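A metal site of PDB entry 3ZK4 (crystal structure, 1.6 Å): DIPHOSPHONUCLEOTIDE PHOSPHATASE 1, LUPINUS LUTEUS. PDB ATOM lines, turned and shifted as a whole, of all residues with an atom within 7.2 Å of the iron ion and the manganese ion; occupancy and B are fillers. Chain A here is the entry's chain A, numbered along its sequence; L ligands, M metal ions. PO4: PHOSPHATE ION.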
ATOM      1  N   GLY A 252      18.295  24.645  -9.146  1.00  0.00           N
ATOM      2  CA  GLY A 252      19.632  24.275  -8.715  1.00  0.00           C
ATOM      3  C   GLY A 252      20.608  24.080  -9.852  1.00  0.00           C
ATOM      4  O   GLY A 252      20.197  23.841 -10.991  1.00  0.00           O
ATOM      5  N   ASP A 253      21.914  24.077  -9.534  1.00  0.00           N
ATOM      6  CA  ASP A 253      22.924  23.343 -10.313  1.00  0.00           C
ATOM      7  C   ASP A 253      23.231  24.041 -11.666  1.00  0.00           C
ATOM      8  O   ASP A 253      23.568  23.370 -12.651  1.00  0.00           O
ATOM      9  CB  ASP A 253      22.506  21.876 -10.584  1.00  0.00           C
ATOM     10  CG  ASP A 253      22.137  21.113  -9.298  1.00  0.00           C
ATOM     11  OD1 ASP A 253      21.102  21.406  -8.682  1.00  0.00           O
ATOM     12  OD2 ASP A 253      22.882  20.220  -8.915  1.00  0.00           O
ATOM     13  N   MET A 254      23.055  25.337 -11.702  1.00  0.00           N
ATOM     14  CA  MET A 254      23.264  26.093 -12.938  1.00  0.00           C
ATOM     15  C   MET A 254      24.717  26.083 -13.396  1.00  0.00           C
ATOM     16  O   MET A 254      24.994  25.925 -14.590  1.00  0.00           O
ATOM     17  CB  MET A 254      22.731  27.521 -12.771  1.00  0.00           C
ATOM     18  CG  MET A 254      22.915  28.364 -14.047  1.00  0.00           C
ATOM     19  SD  MET A 254      22.079  29.941 -14.057  1.00  0.00           S
ATOM     20  CE  MET A 254      23.133  30.844 -12.964  1.00  0.00           C
ATOM     21  N   PHE A 268      31.177  21.547 -17.513  1.00  0.00           N
ATOM     22  CA  PHE A 268      30.143  20.577 -17.794  1.00  0.00           C
ATOM     23  C   PHE A 268      28.779  21.093 -17.393  1.00  0.00           C
ATOM     24  O   PHE A 268      27.922  20.339 -16.921  1.00  0.00           O
ATOM     25  CB  PHE A 268      30.466  19.210 -17.167  1.00  0.00           C
ATOM     26  CG  PHE A 268      30.671  19.231 -15.668  1.00  0.00           C
ATOM     27  CD1 PHE A 268      29.603  19.043 -14.800  1.00  0.00           C
ATOM     28  CD2 PHE A 268      31.947  19.380 -15.135  1.00  0.00           C
ATOM     29  CE1 PHE A 268      29.802  19.033 -13.427  1.00  0.00           C
ATOM     30  CE2 PHE A 268      32.141  19.390 -13.771  1.00  0.00           C
ATOM     31  CZ  PHE A 268      31.073  19.205 -12.917  1.00  0.00           C
ATOM     32  N   ILE A 292      19.557  26.827  -5.533  1.00  0.00           N
ATOM     33  CA  ILE A 292      19.542  25.905  -4.384  1.00  0.00           C
ATOM     34  C   ILE A 292      20.712  24.901  -4.423  1.00  0.00           C
ATOM     35  O   ILE A 292      20.535  23.681  -4.525  1.00  0.00           O
ATOM     36  CB  ILE A 292      18.148  25.313  -4.125  1.00  0.00           C
ATOM     37  CG1 ILE A 292      17.632  24.576  -5.352  1.00  0.00           C
ATOM     38  CG2 ILE A 292      17.207  26.411  -3.687  1.00  0.00           C
ATOM     39  CD1 ILE A 292      16.291  23.895  -5.144  1.00  0.00           C
ATOM     40  N   GLY A 293      21.901  25.448  -4.420  1.00  0.00           N
ATOM     41  CA  GLY A 293      23.125  24.652  -4.342  1.00  0.00           C
ATOM     42  C   GLY A 293      23.691  24.265  -5.706  1.00  0.00           C
ATOM     43  O   GLY A 293      22.942  24.255  -6.718  1.00  0.00           O
ATOM     44  N   ASP A 294      24.959  23.818  -5.655  1.00  0.00           N
ATOM     45  CA  ASP A 294      25.809  23.586  -6.796  1.00  0.00           C
ATOM     46  C   ASP A 294      25.774  24.866  -7.669  1.00  0.00           C
ATOM     47  O   ASP A 294      25.041  24.982  -8.697  1.00  0.00           O
ATOM     48  CB  ASP A 294      25.365  22.350  -7.522  1.00  0.00           C
ATOM     49  CG  ASP A 294      25.798  21.063  -6.841  1.00  0.00           C
ATOM     50  OD1 ASP A 294      26.504  21.104  -5.802  1.00  0.00           O
ATOM     51  OD2 ASP A 294      25.418  20.008  -7.437  1.00  0.00           O
ATOM     52  N   LEU A 295      26.555  25.826  -7.202  1.00  0.00           N
ATOM     53  CA  LEU A 295      26.554  27.200  -7.637  1.00  0.00           C
ATOM     54  C   LEU A 295      27.361  27.352  -8.915  1.00  0.00           C
ATOM     55  O   LEU A 295      26.779  27.641  -9.974  1.00  0.00           O
ATOM     56  CB  LEU A 295      27.061  28.149  -6.525  1.00  0.00           C
ATOM     57  CG  LEU A 295      26.170  28.094  -5.229  1.00  0.00           C
ATOM     58  CD1 LEU A 295      26.713  29.040  -4.178  1.00  0.00           C
ATOM     59  CD2 LEU A 295      24.698  28.368  -5.497  1.00  0.00           C
ATOM     60  N   TYR A 297      30.424  25.172  -9.639  1.00  0.00           N
ATOM     61  CA  TYR A 297      31.248  24.008  -9.936  1.00  0.00           C
ATOM     62  C   TYR A 297      32.736  24.352 -10.138  1.00  0.00           C
ATOM     63  O   TYR A 297      33.474  23.637 -10.846  1.00  0.00           O
ATOM     64  CB  TYR A 297      30.740  23.199 -11.125  1.00  0.00           C
ATOM     65  CG  TYR A 297      29.360  22.559 -10.940  1.00  0.00           C
ATOM     66  CD1 TYR A 297      28.222  23.268 -11.253  1.00  0.00           C
ATOM     67  CD2 TYR A 297      29.223  21.274 -10.421  1.00  0.00           C
ATOM     68  CE1 TYR A 297      26.963  22.684 -11.131  1.00  0.00           C
ATOM     69  CE2 TYR A 297      27.969  20.705 -10.265  1.00  0.00           C
ATOM     70  CZ  TYR A 297      26.847  21.434 -10.610  1.00  0.00           C
ATOM     71  OH  TYR A 297      25.617  20.907 -10.488  1.00  0.00           O
ATOM     72  N   GLY A 326      25.298  23.167  -1.571  1.00  0.00           N
ATOM     73  CA  GLY A 326      25.253  21.786  -1.991  1.00  0.00           C
ATOM     74  C   GLY A 326      26.601  21.067  -1.897  1.00  0.00           C
ATOM     75  O   GLY A 326      27.583  21.586  -1.361  1.00  0.00           O
ATOM     76  N   ASN A 327      26.654  19.881  -2.472  1.00  0.00           N
ATOM     77  CA  ASN A 327      27.853  19.045  -2.302  1.00  0.00           C
ATOM     78  C   ASN A 327      29.074  19.643  -2.955  1.00  0.00           C
ATOM     79  O   ASN A 327      30.191  19.503  -2.447  1.00  0.00           O
ATOM     80  CB  ASN A 327      27.586  17.614  -2.769  1.00  0.00           C
ATOM     81  CG  ASN A 327      27.039  17.520  -4.177  1.00  0.00           C
ATOM     82  OD1 ASN A 327      26.035  18.128  -4.452  1.00  0.00           O
ATOM     83  ND2 ASN A 327      27.643  16.700  -5.019  1.00  0.00           N
ATOM     84  N   HIS A 328      28.889  20.332  -4.096  1.00  0.00           N
ATOM     85  CA  HIS A 328      30.041  20.940  -4.758  1.00  0.00           C
ATOM     86  C   HIS A 328      30.553  22.178  -4.064  1.00  0.00           C
ATOM     87  O   HIS A 328      31.666  22.651  -4.372  1.00  0.00           O
ATOM     88  CB  HIS A 328      29.762  21.198  -6.239  1.00  0.00           C
ATOM     89  CG  HIS A 328      29.742  19.929  -6.989  1.00  0.00           C
ATOM     90  ND1 HIS A 328      30.906  19.299  -7.369  1.00  0.00           N
ATOM     91  CD2 HIS A 328      28.744  19.068  -7.292  1.00  0.00           C
ATOM     92  CE1 HIS A 328      30.631  18.126  -7.916  1.00  0.00           C
ATOM     93  NE2 HIS A 328      29.330  17.973  -7.896  1.00  0.00           N
ATOM     94  N   GLU A 329      29.748  22.755  -3.164  1.00  0.00           N
ATOM     95  CA  GLU A 329      30.269  23.826  -2.319  1.00  0.00           C
ATOM     96  C   GLU A 329      31.039  23.297  -1.125  1.00  0.00           C
ATOM     97  O   GLU A 329      32.037  23.897  -0.699  1.00  0.00           O
ATOM     98  CB  GLU A 329      29.157  24.757  -1.803  1.00  0.00           C
ATOM     99  CG  GLU A 329      28.544  25.674  -2.871  1.00  0.00           C
ATOM    100  CD  GLU A 329      27.758  24.921  -3.883  1.00  0.00           C
ATOM    101  OE1 GLU A 329      26.729  24.290  -3.513  1.00  0.00           O
ATOM    102  OE2 GLU A 329      28.167  24.959  -5.078  1.00  0.00           O
ATOM    103  N   ASP A 343      33.586  16.256  -3.467  1.00  0.00           N
ATOM    104  CA  ASP A 343      32.928  17.078  -4.486  1.00  0.00           C
ATOM    105  C   ASP A 343      33.274  18.584  -4.450  1.00  0.00           C
ATOM    106  O   ASP A 343      33.171  19.261  -5.502  1.00  0.00           O
ATOM    107  CB  ASP A 343      31.423  16.880  -4.432  1.00  0.00           C
ATOM    108  CG  ASP A 343      31.009  15.454  -4.773  1.00  0.00           C
ATOM    109  OD1 ASP A 343      31.882  14.700  -5.255  1.00  0.00           O
ATOM    110  OD2 ASP A 343      29.838  15.101  -4.581  1.00  0.00           O
ATOM    111  N   THR A 382      22.003  20.459   3.004  1.00  0.00           N
ATOM    112  CA  THR A 382      21.986  19.006   2.886  1.00  0.00           C
ATOM    113  C   THR A 382      23.378  18.356   3.035  1.00  0.00           C
ATOM    114  O   THR A 382      23.526  17.150   2.980  1.00  0.00           O
ATOM    115  CB  THR A 382      21.306  18.526   1.595  1.00  0.00           C
ATOM    116  OG1 THR A 382      21.981  19.110   0.485  1.00  0.00           O
ATOM    117  CG2 THR A 382      19.823  18.956   1.564  1.00  0.00           C
ATOM    118  N   GLU A 383      24.393  19.174   3.287  1.00  0.00           N
ATOM    119  CA  GLU A 383      25.745  18.695   3.494  1.00  0.00           C
ATOM    120  C   GLU A 383      26.085  18.647   5.011  1.00  0.00           C
ATOM    121  O   GLU A 383      27.215  18.287   5.374  1.00  0.00           O
ATOM    122  CB  GLU A 383      26.773  19.519   2.731  1.00  0.00           C
ATOM    123  CG  GLU A 383      26.381  19.741   1.253  1.00  0.00           C
ATOM    124  CD  GLU A 383      25.798  18.481   0.570  1.00  0.00           C
ATOM    125  OE1 GLU A 383      26.508  17.418   0.500  1.00  0.00           O
ATOM    126  OE2 GLU A 383      24.636  18.495   0.072  1.00  0.00           O
ATOM    127  N   HIS A 416      19.338  21.369  -1.243  1.00  0.00           N
ATOM    128  CA  HIS A 416      20.080  20.916  -2.421  1.00  0.00           C
ATOM    129  C   HIS A 416      19.861  19.468  -2.770  1.00  0.00           C
ATOM    130  O   HIS A 416      19.187  19.156  -3.771  1.00  0.00           O
ATOM    131  CB  HIS A 416      21.553  21.231  -2.336  1.00  0.00           C
ATOM    132  CG  HIS A 416      22.273  20.768  -3.560  1.00  0.00           C
ATOM    133  ND1 HIS A 416      22.081  21.362  -4.786  1.00  0.00           N
ATOM    134  CD2 HIS A 416      23.119  19.730  -3.785  1.00  0.00           C
ATOM    135  CE1 HIS A 416      22.781  20.734  -5.710  1.00  0.00           C
ATOM    136  NE2 HIS A 416      23.441  19.759  -5.126  1.00  0.00           N
ATOM    137  N   ARG A 417      20.406  18.530  -1.978  1.00  0.00           N
ATOM    138  CA  ARG A 417      20.141  17.140  -2.228  1.00  0.00           C
ATOM    139  C   ARG A 417      18.687  16.792  -2.027  1.00  0.00           C
ATOM    140  O   ARG A 417      17.944  17.495  -1.367  1.00  0.00           O
ATOM    141  CB  ARG A 417      21.067  16.250  -1.352  1.00  0.00           C
ATOM    142  CG  ARG A 417      22.566  16.389  -1.585  1.00  0.00           C
ATOM    143  CD  ARG A 417      23.304  15.548  -0.561  1.00  0.00           C
ATOM    144  NE  ARG A 417      24.736  15.480  -0.762  1.00  0.00           N
ATOM    145  CZ  ARG A 417      25.339  14.603  -1.539  1.00  0.00           C
ATOM    146  NH1 ARG A 417      24.636  13.670  -2.173  1.00  0.00           N
ATOM    147  NH2 ARG A 417      26.656  14.580  -1.619  1.00  0.00           N
ATOM    148  N   GLY A 457      17.497  20.536  -5.704  1.00  0.00           N
ATOM    149  CA  GLY A 457      18.382  20.520  -6.851  1.00  0.00           C
ATOM    150  C   GLY A 457      19.047  19.134  -6.939  1.00  0.00           C
ATOM    151  O   GLY A 457      18.383  18.085  -6.746  1.00  0.00           O
ATOM    152  N   HIS A 458      20.328  19.144  -7.302  1.00  0.00           N
ATOM    153  CA  HIS A 458      21.262  17.994  -7.224  1.00  0.00           C
ATOM    154  C   HIS A 458      21.073  16.965  -8.338  1.00  0.00           C
ATOM    155  O   HIS A 458      22.052  16.537  -8.923  1.00  0.00           O
ATOM    156  CB  HIS A 458      21.178  17.344  -5.824  1.00  0.00           C
ATOM    157  CG  HIS A 458      22.174  16.268  -5.610  1.00  0.00           C
ATOM    158  ND1 HIS A 458      23.521  16.491  -5.634  1.00  0.00           N
ATOM    159  CD2 HIS A 458      22.022  14.954  -5.356  1.00  0.00           C
ATOM    160  CE1 HIS A 458      24.167  15.366  -5.388  1.00  0.00           C
ATOM    161  NE2 HIS A 458      23.272  14.420  -5.219  1.00  0.00           N
ATOM    162  N   VAL A 459      19.842  16.521  -8.553  1.00  0.00           N
ATOM    163  CA  VAL A 459      19.487  15.687  -9.691  1.00  0.00           C
ATOM    164  C   VAL A 459      19.260  16.602 -10.874  1.00  0.00           C
ATOM    165  O   VAL A 459      18.394  17.485 -10.833  1.00  0.00           O
ATOM    166  CB  VAL A 459      18.228  14.870  -9.393  1.00  0.00           C
ATOM    167  CG1 VAL A 459      17.817  14.138 -10.631  1.00  0.00           C
ATOM    168  CG2 VAL A 459      18.520  13.868  -8.253  1.00  0.00           C
ATOM    169  N   HIS A 460      20.037  16.402 -11.936  1.00  0.00           N
ATOM    170  CA  HIS A 460      19.993  17.374 -13.074  1.00  0.00           C
ATOM    171  C   HIS A 460      18.867  17.052 -14.055  1.00  0.00           C
ATOM    172  O   HIS A 460      19.116  16.562 -15.182  1.00  0.00           O
ATOM    173  CB  HIS A 460      21.351  17.426 -13.775  1.00  0.00           C
ATOM    174  CG  HIS A 460      22.482  17.802 -12.868  1.00  0.00           C
ATOM    175  ND1 HIS A 460      23.796  17.451 -13.093  1.00  0.00           N
ATOM    176  CD2 HIS A 460      22.479  18.481 -11.683  1.00  0.00           C
ATOM    177  CE1 HIS A 460      24.544  17.906 -12.114  1.00  0.00           C
ATOM    178  NE2 HIS A 460      23.769  18.518 -11.243  1.00  0.00           N
ATOM    179  N   GLY A 494      16.744  20.566 -10.471  1.00  0.00           N
ATOM    180  CA  GLY A 494      18.177  20.571 -10.585  1.00  0.00           C
ATOM    181  C   GLY A 494      18.686  20.685 -12.007  1.00  0.00           C
ATOM    182  O   GLY A 494      19.888  20.525 -12.223  1.00  0.00           O
ATOM    183  N   ALA A 498      23.997  22.131 -15.256  1.00  0.00           N
ATOM    184  CA  ALA A 498      24.888  20.988 -15.219  1.00  0.00           C
ATOM    185  C   ALA A 498      24.360  19.751 -15.971  1.00  0.00           C
ATOM    186  O   ALA A 498      23.146  19.509 -16.018  1.00  0.00           O
ATOM    187  CB  ALA A 498      25.179  20.598 -13.740  1.00  0.00           C
ATOM    188  N   SER A 499      25.278  18.993 -16.545  1.00  0.00           N
ATOM    189  CA  SER A 499      24.998  17.778 -17.347  1.00  0.00           C
ATOM    190  C   SER A 499      23.796  16.989 -16.868  1.00  0.00           C
ATOM    191  O   SER A 499      23.728  16.614 -15.705  1.00  0.00           O
ATOM    192  CB  SER A 499      26.185  16.832 -17.297  1.00  0.00           C
ATOM    193  OG  SER A 499      27.343  17.498 -17.611  1.00  0.00           O
HETATM  194  P   PO4 L   1      25.677  16.950  -8.667  1.00  0.00           P
HETATM  195  O1  PO4 L   1      26.411  17.933  -9.568  1.00  0.00           O
HETATM  196  O2  PO4 L   1      24.267  17.599  -8.416  1.00  0.00           O
HETATM  197  O3  PO4 L   1      26.357  16.851  -7.351  1.00  0.00           O
HETATM  198  O4  PO4 L   1      25.355  15.586  -9.318  1.00  0.00           O
HETATM  199 FE    FE M   1      24.713  19.517  -9.534  1.00  0.00          FE
HETATM  200 MN    MN M   2      24.714  18.293  -6.100  1.00  0.00          MN
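The iron ion is bound by OH of Tyr 297, OD2 of Asp 253, NE2 of His 460, O2 of the ligand, OD2 of Asp 294 and O1 of the ligand.
Within 4 Å of the manganese ion: Asp 253, Asp 294, Asn 327, His 416 and His 458.
Along chain A the residues within 4 Å of the iron ion span positions 253 to 460.
The manganese ion is bound by the side-chain amide oxygen (OD1) of Asn 327 (2.1 Å), a ring nitrogen (NE2) of His 416 (2.2 Å), a ring nitrogen (ND1) of His 458 (2.2 Å), the side-chain carboxylate (OD2) of Asp 294 (2.3 Å), an oxygen (O2) of the ligand (2.5 Å) and an oxygen (O3) of the ligand (2.5 Å). The manganese ion has six donor atoms within binding distance.
OD1 of Asp 253 sits at hydrogen-bond distance from N of His 458. The backbone NH (N) of Ala 498 is in hydrogen-bond range of the backbone carbonyl oxygen (O) of Asp 253, at 2.9 Å. The backbone NH of Asp 253 lies within hydrogen-bond range of the backbone carbonyl oxygen of Gly 293 (3.0 Å). The side-chain amide nitrogen of Asn 327 lies within hydrogen-bond range of the side-chain carboxylate of Asp 343. The backbone NH (N) of Gly 457 is in hydrogen-bond range of the backbone carbonyl oxygen (O) of His 416 (2.9 Å). A ring nitrogen (ND1) of His 460 is in hydrogen-bond range of the backbone carbonyl oxygen (O) of Ser 499 (2.7 Å). The backbone NH of His 328 sits at hydrogen-bond distance from the side-chain carboxylate of Asp 294, at 3.0 Å. The backbone NH (N) of Asp 294 lies within hydrogen-bond range of the side-chain carboxylate (OE1) of Glu 329 (2.8 Å).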
